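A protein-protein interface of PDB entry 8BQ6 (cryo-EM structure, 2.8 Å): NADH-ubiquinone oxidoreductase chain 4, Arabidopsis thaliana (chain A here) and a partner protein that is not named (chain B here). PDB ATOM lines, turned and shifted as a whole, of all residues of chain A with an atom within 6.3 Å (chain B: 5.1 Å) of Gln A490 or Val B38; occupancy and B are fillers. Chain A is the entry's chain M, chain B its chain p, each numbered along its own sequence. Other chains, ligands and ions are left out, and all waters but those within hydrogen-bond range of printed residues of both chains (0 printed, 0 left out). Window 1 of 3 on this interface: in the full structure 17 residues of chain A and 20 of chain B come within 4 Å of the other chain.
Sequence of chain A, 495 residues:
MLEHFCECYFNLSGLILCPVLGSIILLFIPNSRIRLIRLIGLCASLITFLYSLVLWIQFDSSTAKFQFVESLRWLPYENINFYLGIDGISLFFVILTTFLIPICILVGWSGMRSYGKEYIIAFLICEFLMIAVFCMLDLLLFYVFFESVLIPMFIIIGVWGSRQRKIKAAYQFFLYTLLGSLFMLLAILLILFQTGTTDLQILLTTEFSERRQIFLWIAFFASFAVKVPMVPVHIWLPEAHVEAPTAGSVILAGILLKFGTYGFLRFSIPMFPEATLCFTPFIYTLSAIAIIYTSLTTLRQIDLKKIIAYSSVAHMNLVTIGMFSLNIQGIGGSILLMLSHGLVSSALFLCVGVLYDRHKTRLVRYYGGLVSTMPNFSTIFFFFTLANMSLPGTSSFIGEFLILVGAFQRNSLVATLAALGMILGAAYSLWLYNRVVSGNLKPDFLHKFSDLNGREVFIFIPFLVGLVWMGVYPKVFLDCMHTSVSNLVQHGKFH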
ATOM      1  N   HIS A 482       7.148  -3.485  26.402  1.00  0.00           N
ATOM      2  CA  HIS A 482       7.992  -2.724  25.486  1.00  0.00           C
ATOM      3  C   HIS A 482       7.187  -1.961  24.443  1.00  0.00           C
ATOM      4  O   HIS A 482       7.631  -0.916  23.956  1.00  0.00           O
ATOM      5  CB  HIS A 482       8.994  -3.650  24.801  1.00  0.00           C
ATOM      6  CG  HIS A 482      10.254  -3.845  25.582  1.00  0.00           C
ATOM      7  ND1 HIS A 482      11.038  -4.971  25.463  1.00  0.00           N
ATOM      8  CD2 HIS A 482      10.850  -3.067  26.514  1.00  0.00           C
ATOM      9  CE1 HIS A 482      12.074  -4.870  26.276  1.00  0.00           C
ATOM     10  NE2 HIS A 482      11.983  -3.724  26.926  1.00  0.00           N
ATOM     11  N   THR A 483       6.013  -2.469  24.069  1.00  0.00           N
ATOM     12  CA  THR A 483       5.219  -1.782  23.054  1.00  0.00           C
ATOM     13  C   THR A 483       4.625  -0.492  23.605  1.00  0.00           C
ATOM     14  O   THR A 483       4.590   0.534  22.917  1.00  0.00           O
ATOM     15  CB  THR A 483       4.116  -2.698  22.532  1.00  0.00           C
ATOM     16  OG1 THR A 483       4.680  -3.956  22.146  1.00  0.00           O
ATOM     17  CG2 THR A 483       3.447  -2.066  21.326  1.00  0.00           C
ATOM     18  N   VAL A 485       5.918   1.058  26.285  1.00  0.00           N
ATOM     19  CA  VAL A 485       7.079   1.887  26.591  1.00  0.00           C
ATOM     20  C   VAL A 485       7.578   2.582  25.333  1.00  0.00           C
ATOM     21  O   VAL A 485       7.913   3.771  25.355  1.00  0.00           O
ATOM     22  CB  VAL A 485       8.184   1.041  27.249  1.00  0.00           C
ATOM     23  CG1 VAL A 485       9.518   1.772  27.192  1.00  0.00           C
ATOM     24  CG2 VAL A 485       7.819   0.717  28.683  1.00  0.00           C
ATOM     25  N   SER A 486       7.622   1.855  24.215  1.00  0.00           N
ATOM     26  CA  SER A 486       8.146   2.428  22.980  1.00  0.00           C
ATOM     27  C   SER A 486       7.305   3.606  22.518  1.00  0.00           C
ATOM     28  O   SER A 486       7.841   4.640  22.103  1.00  0.00           O
ATOM     29  CB  SER A 486       8.202   1.358  21.896  1.00  0.00           C
ATOM     30  OG  SER A 486       9.202   0.404  22.194  1.00  0.00           O
ATOM     31  N   ASN A 487       5.982   3.471  22.592  1.00  0.00           N
ATOM     32  CA  ASN A 487       5.099   4.531  22.130  1.00  0.00           C
ATOM     33  C   ASN A 487       5.063   5.697  23.104  1.00  0.00           C
ATOM     34  O   ASN A 487       4.786   6.833  22.703  1.00  0.00           O
ATOM     35  CB  ASN A 487       3.705   3.961  21.903  1.00  0.00           C
ATOM     36  CG  ASN A 487       3.535   3.411  20.510  1.00  0.00           C
ATOM     37  OD1 ASN A 487       3.718   2.219  20.275  1.00  0.00           O
ATOM     38  ND2 ASN A 487       3.182   4.274  19.575  1.00  0.00           N
ATOM     39  N   LEU A 488       5.372   5.445  24.374  1.00  0.00           N
ATOM     40  CA  LEU A 488       5.460   6.560  25.353  1.00  0.00           C
ATOM     41  C   LEU A 488       6.688   7.402  25.015  1.00  0.00           C
ATOM     42  O   LEU A 488       6.595   8.638  25.090  1.00  0.00           O
ATOM     43  CB  LEU A 488       5.549   5.975  26.766  1.00  0.00           C
ATOM     44  CG  LEU A 488       5.966   6.930  27.880  1.00  0.00           C
ATOM     45  CD1 LEU A 488       4.863   7.931  28.167  1.00  0.00           C
ATOM     46  CD2 LEU A 488       6.301   6.149  29.134  1.00  0.00           C
ATOM     47  N   VAL A 489       7.788   6.749  24.635  1.00  0.00           N
ATOM     48  CA  VAL A 489       9.013   7.476  24.329  1.00  0.00           C
ATOM     49  C   VAL A 489       8.843   8.280  23.047  1.00  0.00           C
ATOM     50  O   VAL A 489       9.329   9.412  22.931  1.00  0.00           O
ATOM     51  CB  VAL A 489      10.184   6.483  24.221  1.00  0.00           C
ATOM     52  CG1 VAL A 489      11.454   7.190  23.808  1.00  0.00           C
ATOM     53  CG2 VAL A 489      10.357   5.718  25.519  1.00  0.00           C
ATOM     54  N   GLN A 490       8.150   7.706  22.067  1.00  0.00           N
ATOM     55  CA  GLN A 490       7.996   8.327  20.763  1.00  0.00           C
ATOM     56  C   GLN A 490       6.925   9.408  20.754  1.00  0.00           C
ATOM     57  O   GLN A 490       6.837  10.172  19.786  1.00  0.00           O
ATOM     58  CB  GLN A 490       7.677   7.243  19.729  1.00  0.00           C
ATOM     59  CG  GLN A 490       7.601   7.722  18.300  1.00  0.00           C
ATOM     60  CD  GLN A 490       8.955   8.105  17.762  1.00  0.00           C
ATOM     61  OE1 GLN A 490       9.954   7.438  18.027  1.00  0.00           O
ATOM     62  NE2 GLN A 490       8.999   9.185  16.996  1.00  0.00           N
ATOM     63  N   HIS A 491       6.159   9.510  21.835  1.00  0.00           N
ATOM     64  CA  HIS A 491       5.008  10.446  21.869  1.00  0.00           C
ATOM     65  C   HIS A 491       5.464  11.893  21.718  1.00  0.00           C
ATOM     66  O   HIS A 491       6.221  12.372  22.584  1.00  0.00           O
ATOM     67  CB  HIS A 491       4.194  10.225  23.143  1.00  0.00           C
ATOM     68  CG  HIS A 491       2.802  10.729  23.026  1.00  0.00           C
ATOM     69  ND1 HIS A 491       1.752   9.905  22.695  1.00  0.00           N
ATOM     70  CD2 HIS A 491       2.292  11.970  23.160  1.00  0.00           C
ATOM     71  CE1 HIS A 491       0.648  10.615  22.643  1.00  0.00           C
ATOM     72  NE2 HIS A 491       0.953  11.883  22.933  1.00  0.00           N
ATOM     73  N   GLY A 492       4.977  12.566  20.678  1.00  0.00           N
ATOM     74  CA  GLY A 492       5.329  13.945  20.439  1.00  0.00           C
ATOM     75  C   GLY A 492       6.401  14.157  19.393  1.00  0.00           C
ATOM     76  O   GLY A 492       6.731  15.310  19.099  1.00  0.00           O
ATOM     77  N   LYS A 493       6.965  13.088  18.837  1.00  0.00           N
ATOM     78  CA  LYS A 493       7.946  13.192  17.766  1.00  0.00           C
ATOM     79  C   LYS A 493       7.518  12.309  16.606  1.00  0.00           C
ATOM     80  O   LYS A 493       6.799  11.322  16.785  1.00  0.00           O
ATOM     81  CB  LYS A 493       9.364  12.799  18.222  1.00  0.00           C
ATOM     82  CG  LYS A 493       9.637  12.936  19.710  1.00  0.00           C
ATOM     83  CD  LYS A 493      11.095  12.611  20.037  1.00  0.00           C
ATOM     84  CE  LYS A 493      12.065  13.454  19.210  1.00  0.00           C
ATOM     85  NZ  LYS A 493      13.477  12.966  19.266  1.00  0.00           N
ATOM     86  N   PHE A 494       7.975  12.669  15.410  1.00  0.00           N
ATOM     87  CA  PHE A 494       7.581  11.980  14.188  1.00  0.00           C
ATOM     88  C   PHE A 494       8.787  11.696  13.314  1.00  0.00           C
ATOM     89  O   PHE A 494       8.712  11.711  12.083  1.00  0.00           O
ATOM     90  CB  PHE A 494       6.528  12.783  13.437  1.00  0.00           C
ATOM     91  CG  PHE A 494       5.305  13.038  14.249  1.00  0.00           C
ATOM     92  CD1 PHE A 494       4.340  12.060  14.382  1.00  0.00           C
ATOM     93  CD2 PHE A 494       5.136  14.235  14.915  1.00  0.00           C
ATOM     94  CE1 PHE A 494       3.218  12.280  15.145  1.00  0.00           C
ATOM     95  CE2 PHE A 494       4.019  14.453  15.685  1.00  0.00           C
ATOM     96  CZ  PHE A 494       3.055  13.478  15.793  1.00  0.00           C
ATOM     97  N   HIS A 495       9.916  11.416  13.948  1.00  0.00           N
ATOM     98  CA  HIS A 495      11.112  11.014  13.234  1.00  0.00           C
ATOM     99  C   HIS A 495      11.920  10.073  14.114  1.00  0.00           C
ATOM    100  O   HIS A 495      11.605   9.901  15.291  1.00  0.00           O
ATOM    101  CB  HIS A 495      11.936  12.236  12.838  1.00  0.00           C
ATOM    102  CG  HIS A 495      12.298  13.120  13.991  1.00  0.00           C
ATOM    103  ND1 HIS A 495      11.803  14.397  14.132  1.00  0.00           N
ATOM    104  CD2 HIS A 495      13.111  12.910  15.053  1.00  0.00           C
ATOM    105  CE1 HIS A 495      12.293  14.937  15.234  1.00  0.00           C
ATOM    106  NE2 HIS A 495      13.090  14.055  15.810  1.00  0.00           N
ATOM    107  N   MET B  33       0.533   7.153  12.723  1.00  0.00           N
ATOM    108  CA  MET B  33       1.922   7.403  12.350  1.00  0.00           C
ATOM    109  C   MET B  33       2.860   7.106  13.511  1.00  0.00           C
ATOM    110  O   MET B  33       3.950   6.558  13.315  1.00  0.00           O
ATOM    111  CB  MET B  33       2.091   8.849  11.884  1.00  0.00           C
ATOM    112  CG  MET B  33       3.358   9.120  11.086  1.00  0.00           C
ATOM    113  SD  MET B  33       3.645   7.943   9.754  1.00  0.00           S
ATOM    114  CE  MET B  33       3.156   8.923   8.338  1.00  0.00           C
ATOM    115  N   ARG B  34       2.452   7.461  14.729  1.00  0.00           N
ATOM    116  CA  ARG B  34       3.295   7.198  15.889  1.00  0.00           C
ATOM    117  C   ARG B  34       3.508   5.700  16.082  1.00  0.00           C
ATOM    118  O   ARG B  34       4.630   5.250  16.338  1.00  0.00           O
ATOM    119  CB  ARG B  34       2.676   7.835  17.131  1.00  0.00           C
ATOM    120  CG  ARG B  34       3.562   7.781  18.353  1.00  0.00           C
ATOM    121  CD  ARG B  34       2.745   7.951  19.610  1.00  0.00           C
ATOM    122  NE  ARG B  34       1.965   6.754  19.882  1.00  0.00           N
ATOM    123  CZ  ARG B  34       0.713   6.752  20.314  1.00  0.00           C
ATOM    124  NH1 ARG B  34       0.074   7.876  20.585  1.00  0.00           N
ATOM    125  NH2 ARG B  34       0.088   5.590  20.479  1.00  0.00           N
ATOM    126  N   GLU B  35       2.439   4.908  15.944  1.00  0.00           N
ATOM    127  CA  GLU B  35       2.569   3.457  16.045  1.00  0.00           C
ATOM    128  C   GLU B  35       3.415   2.895  14.913  1.00  0.00           C
ATOM    129  O   GLU B  35       4.210   1.971  15.119  1.00  0.00           O
ATOM    130  CB  GLU B  35       1.195   2.794  16.028  1.00  0.00           C
ATOM    131  CG  GLU B  35       0.123   3.574  16.725  1.00  0.00           C
ATOM    132  CD  GLU B  35      -0.113   3.103  18.128  1.00  0.00           C
ATOM    133  OE1 GLU B  35      -0.567   3.919  18.955  1.00  0.00           O
ATOM    134  OE2 GLU B  35       0.141   1.912  18.392  1.00  0.00           O
ATOM    135  N   HIS B  36       3.229   3.422  13.701  1.00  0.00           N
ATOM    136  CA  HIS B  36       3.982   2.934  12.550  1.00  0.00           C
ATOM    137  C   HIS B  36       5.468   3.230  12.698  1.00  0.00           C
ATOM    138  O   HIS B  36       6.311   2.405  12.329  1.00  0.00           O
ATOM    139  CB  HIS B  36       3.423   3.552  11.269  1.00  0.00           C
ATOM    140  CG  HIS B  36       4.196   3.205  10.034  1.00  0.00           C
ATOM    141  ND1 HIS B  36       3.910   2.100   9.263  1.00  0.00           N
ATOM    142  CD2 HIS B  36       5.232   3.830   9.426  1.00  0.00           C
ATOM    143  CE1 HIS B  36       4.743   2.054   8.238  1.00  0.00           C
ATOM    144  NE2 HIS B  36       5.555   3.093   8.314  1.00  0.00           N
ATOM    145  N   ILE B  37       5.810   4.405  13.233  1.00  0.00           N
ATOM    146  CA  ILE B  37       7.216   4.743  13.447  1.00  0.00           C
ATOM    147  C   ILE B  37       7.825   3.846  14.514  1.00  0.00           C
ATOM    148  O   ILE B  37       8.979   3.416  14.399  1.00  0.00           O
ATOM    149  CB  ILE B  37       7.365   6.228  13.821  1.00  0.00           C
ATOM    150  CG1 ILE B  37       7.011   7.119  12.639  1.00  0.00           C
ATOM    151  CG2 ILE B  37       8.786   6.519  14.264  1.00  0.00           C
ATOM    152  CD1 ILE B  37       6.704   8.526  13.053  1.00  0.00           C
ATOM    153  N   VAL B  38       7.070   3.569  15.581  1.00  0.00           N
ATOM    154  CA  VAL B  38       7.567   2.678  16.625  1.00  0.00           C
ATOM    155  C   VAL B  38       7.874   1.308  16.039  1.00  0.00           C
ATOM    156  O   VAL B  38       8.935   0.727  16.295  1.00  0.00           O
ATOM    157  CB  VAL B  38       6.552   2.582  17.778  1.00  0.00           C
ATOM    158  CG1 VAL B  38       6.825   1.349  18.623  1.00  0.00           C
ATOM    159  CG2 VAL B  38       6.586   3.841  18.626  1.00  0.00           C
ATOM    160  N   ARG B  39       6.956   0.785  15.226  1.00  0.00           N
ATOM    161  CA  ARG B  39       7.170  -0.513  14.600  1.00  0.00           C
ATOM    162  C   ARG B  39       8.350  -0.473  13.643  1.00  0.00           C
ATOM    163  O   ARG B  39       9.137  -1.425  13.574  1.00  0.00           O
ATOM    164  CB  ARG B  39       5.906  -0.950  13.870  1.00  0.00           C
ATOM    165  CG  ARG B  39       4.826  -1.465  14.784  1.00  0.00           C
ATOM    166  CD  ARG B  39       3.648  -1.926  13.974  1.00  0.00           C
ATOM    167  NE  ARG B  39       2.468  -1.108  14.211  1.00  0.00           N
ATOM    168  CZ  ARG B  39       1.836  -0.421  13.270  1.00  0.00           C
ATOM    169  NH1 ARG B  39       2.275  -0.392  12.022  1.00  0.00           N
ATOM    170  NH2 ARG B  39       0.734   0.251  13.588  1.00  0.00           N
ATOM    171  N   GLU B  40       8.482   0.614  12.884  1.00  0.00           N
ATOM    172  CA  GLU B  40       9.608   0.739  11.969  1.00  0.00           C
ATOM    173  C   GLU B  40      10.925   0.802  12.731  1.00  0.00           C
ATOM    174  O   GLU B  40      11.907   0.155  12.351  1.00  0.00           O
ATOM    175  CB  GLU B  40       9.426   1.971  11.085  1.00  0.00           C
ATOM    176  CG  GLU B  40       9.764   1.725   9.629  1.00  0.00           C
ATOM    177  CD  GLU B  40       8.891   0.655   9.008  1.00  0.00           C
ATOM    178  OE1 GLU B  40       9.335   0.015   8.033  1.00  0.00           O
ATOM    179  OE2 GLU B  40       7.755   0.459   9.489  1.00  0.00           O
ATOM    180  N   LYS B  41      10.957   1.558  13.830  1.00  0.00           N
ATOM    181  CA  LYS B  41      12.181   1.651  14.617  1.00  0.00           C
ATOM    182  C   LYS B  41      12.560   0.299  15.203  1.00  0.00           C
ATOM    183  O   LYS B  41      13.747  -0.034  15.295  1.00  0.00           O
ATOM    184  CB  LYS B  41      12.027   2.697  15.720  1.00  0.00           C
ATOM    185  CG  LYS B  41      12.088   4.113  15.198  1.00  0.00           C
ATOM    186  CD  LYS B  41      12.023   5.158  16.292  1.00  0.00           C
ATOM    187  CE  LYS B  41      12.204   6.538  15.678  1.00  0.00           C
ATOM    188  NZ  LYS B  41      12.680   7.570  16.637  1.00  0.00           N
ATOM    189  N   TRP B  42      11.566  -0.501  15.590  1.00  0.00           N
ATOM    190  CA  TRP B  42      11.857  -1.821  16.140  1.00  0.00           C
ATOM    191  C   TRP B  42      12.406  -2.762  15.077  1.00  0.00           C
ATOM    192  O   TRP B  42      13.150  -3.697  15.396  1.00  0.00           O
ATOM    193  CB  TRP B  42      10.607  -2.412  16.786  1.00  0.00           C
ATOM    194  CG  TRP B  42      10.476  -2.034  18.221  1.00  0.00           C
ATOM    195  CD1 TRP B  42       9.635  -1.104  18.747  1.00  0.00           C
ATOM    196  CD2 TRP B  42      11.222  -2.569  19.319  1.00  0.00           C
ATOM    197  NE1 TRP B  42       9.805  -1.027  20.107  1.00  0.00           N
ATOM    198  CE2 TRP B  42      10.776  -1.914  20.482  1.00  0.00           C
ATOM    199  CE3 TRP B  42      12.224  -3.534  19.430  1.00  0.00           C
ATOM    200  CZ2 TRP B  42      11.293  -2.198  21.740  1.00  0.00           C
ATOM    201  CZ3 TRP B  42      12.737  -3.813  20.680  1.00  0.00           C
ATOM    202  CH2 TRP B  42      12.268  -3.150  21.819  1.00  0.00           C
ATOM    203  N   TRP B  86      16.301   4.431  20.216  1.00  0.00           N
ATOM    204  CA  TRP B  86      16.123   5.685  20.934  1.00  0.00           C
ATOM    205  C   TRP B  86      17.367   6.032  21.746  1.00  0.00           C
ATOM    206  O   TRP B  86      17.277   6.669  22.796  1.00  0.00           O
ATOM    207  CB  TRP B  86      14.890   5.612  21.832  1.00  0.00           C
ATOM    208  CG  TRP B  86      13.570   5.448  21.114  1.00  0.00           C
ATOM    209  CD1 TRP B  86      12.678   6.433  20.805  1.00  0.00           C
ATOM    210  CD2 TRP B  86      12.991   4.225  20.639  1.00  0.00           C
ATOM    211  NE1 TRP B  86      11.582   5.901  20.171  1.00  0.00           N
ATOM    212  CE2 TRP B  86      11.752   4.548  20.054  1.00  0.00           C
ATOM    213  CE3 TRP B  86      13.404   2.891  20.646  1.00  0.00           C
ATOM    214  CZ2 TRP B  86      10.922   3.588  19.487  1.00  0.00           C
ATOM    215  CZ3 TRP B  86      12.576   1.941  20.088  1.00  0.00           C
ATOM    216  CH2 TRP B  86      11.352   2.293  19.512  1.00  0.00           C
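The backbone carbonyl oxygen (O) of His A495 is in hydrogen-bond range of the side-chain amino group (NZ) of Lys B41, at 2.9 Å.
The side-chain amide nitrogen (ND2) of Asn A487 lies close to the guanidinium group (NE) of Arg B34 (2.8 Å).
The indole nitrogen (NE1) of Trp B86 sits at hydrogen-bond distance from the side-chain amide oxygen (OE1) of Gln A490.
The side-chain hydroxyl (OG) of Ser A486 is in hydrogen-bond range of the indole nitrogen (NE1) of Trp B42, at 2.6 Å.
NH1 of Arg B34 lies within hydrogen-bond range of ND1 of His A491.
The side-chain amino group of Lys B41 lies within hydrogen-bond range of the side-chain amide oxygen of Gln A490, at 3.1 Å.
Among the printed residues, pairs that only touch across the chains: Val A489 with Trp B86 (3.3 Å), Ser A486 with Val B38 (3.6 Å), Asn A487 with Val B38 (3.6 Å), Asn A487 with Glu B35 (3.7 Å), Gln A490 with Val B38 (3.7 Å), Phe A494 with Ile B37 (3.7 Å), Gln A490 with Ile B37 (3.8 Å) and Ser A486 with Trp B86 (3.9 Å).
The side-chain amide oxygen (OD1) of Asn A487 lies close to the backbone carbonyl oxygen (O) of Thr A483 (3.3 Å).
NE2 of Gln A490 lies within hydrogen-bond range of O of Lys A493 (3.1 Å).
NE of Arg B34 is in salt-bridge range of OE1 of Glu B35, 3.9 Å away.
The backbone carbonyl oxygen (O) of His A482 sits at hydrogen-bond distance from the side-chain hydroxyl (OG) of Ser A486.
NE2 of Gln A490 lies within hydrogen-bond range of O of His A495 (3.2 Å).
Of the 11 printed residues of chain B, 7 touch a printed residue of chain A.
Hydrophobic or aromatic side chains of chain B within 4 Å of the printed part of chain A: Ile B37, Val B38, Trp B42 and Trp B86.
Hydrophobic or aromatic side chains of chain A that line the printed part of chain B: Val A489 and His A491.
Among the printed residues, 14 pairs touch across the chains.
Among the printed residues, no Asp or Glu carboxylate lies within 4 Å of a Lys or Arg side-chain nitrogen of the other chain.
Of the printed residues of chain B, Ser A486 touches Val B38, Trp B42 and Trp B86.
Gln A490 touches just these residues of chain B: Ile B37, Val B38, Lys B41 and Trp B86.
Printed residues of chain A within 4 Å of Ile B37: Gln A490 (3.8 Å) and Phe A494 (3.7 Å).
Glu B40 touches none of the printed residues of chain A.
The nearest residue of chain B that does not touch Gln A490 is Arg B34 (4.04 Å).
The nearest residue of chain A that does not touch Val B38 is Thr A483 (4.9 Å).
The nearest printed residue of chain B that does not touch Val A489 is Val B38 (6.7 Å).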
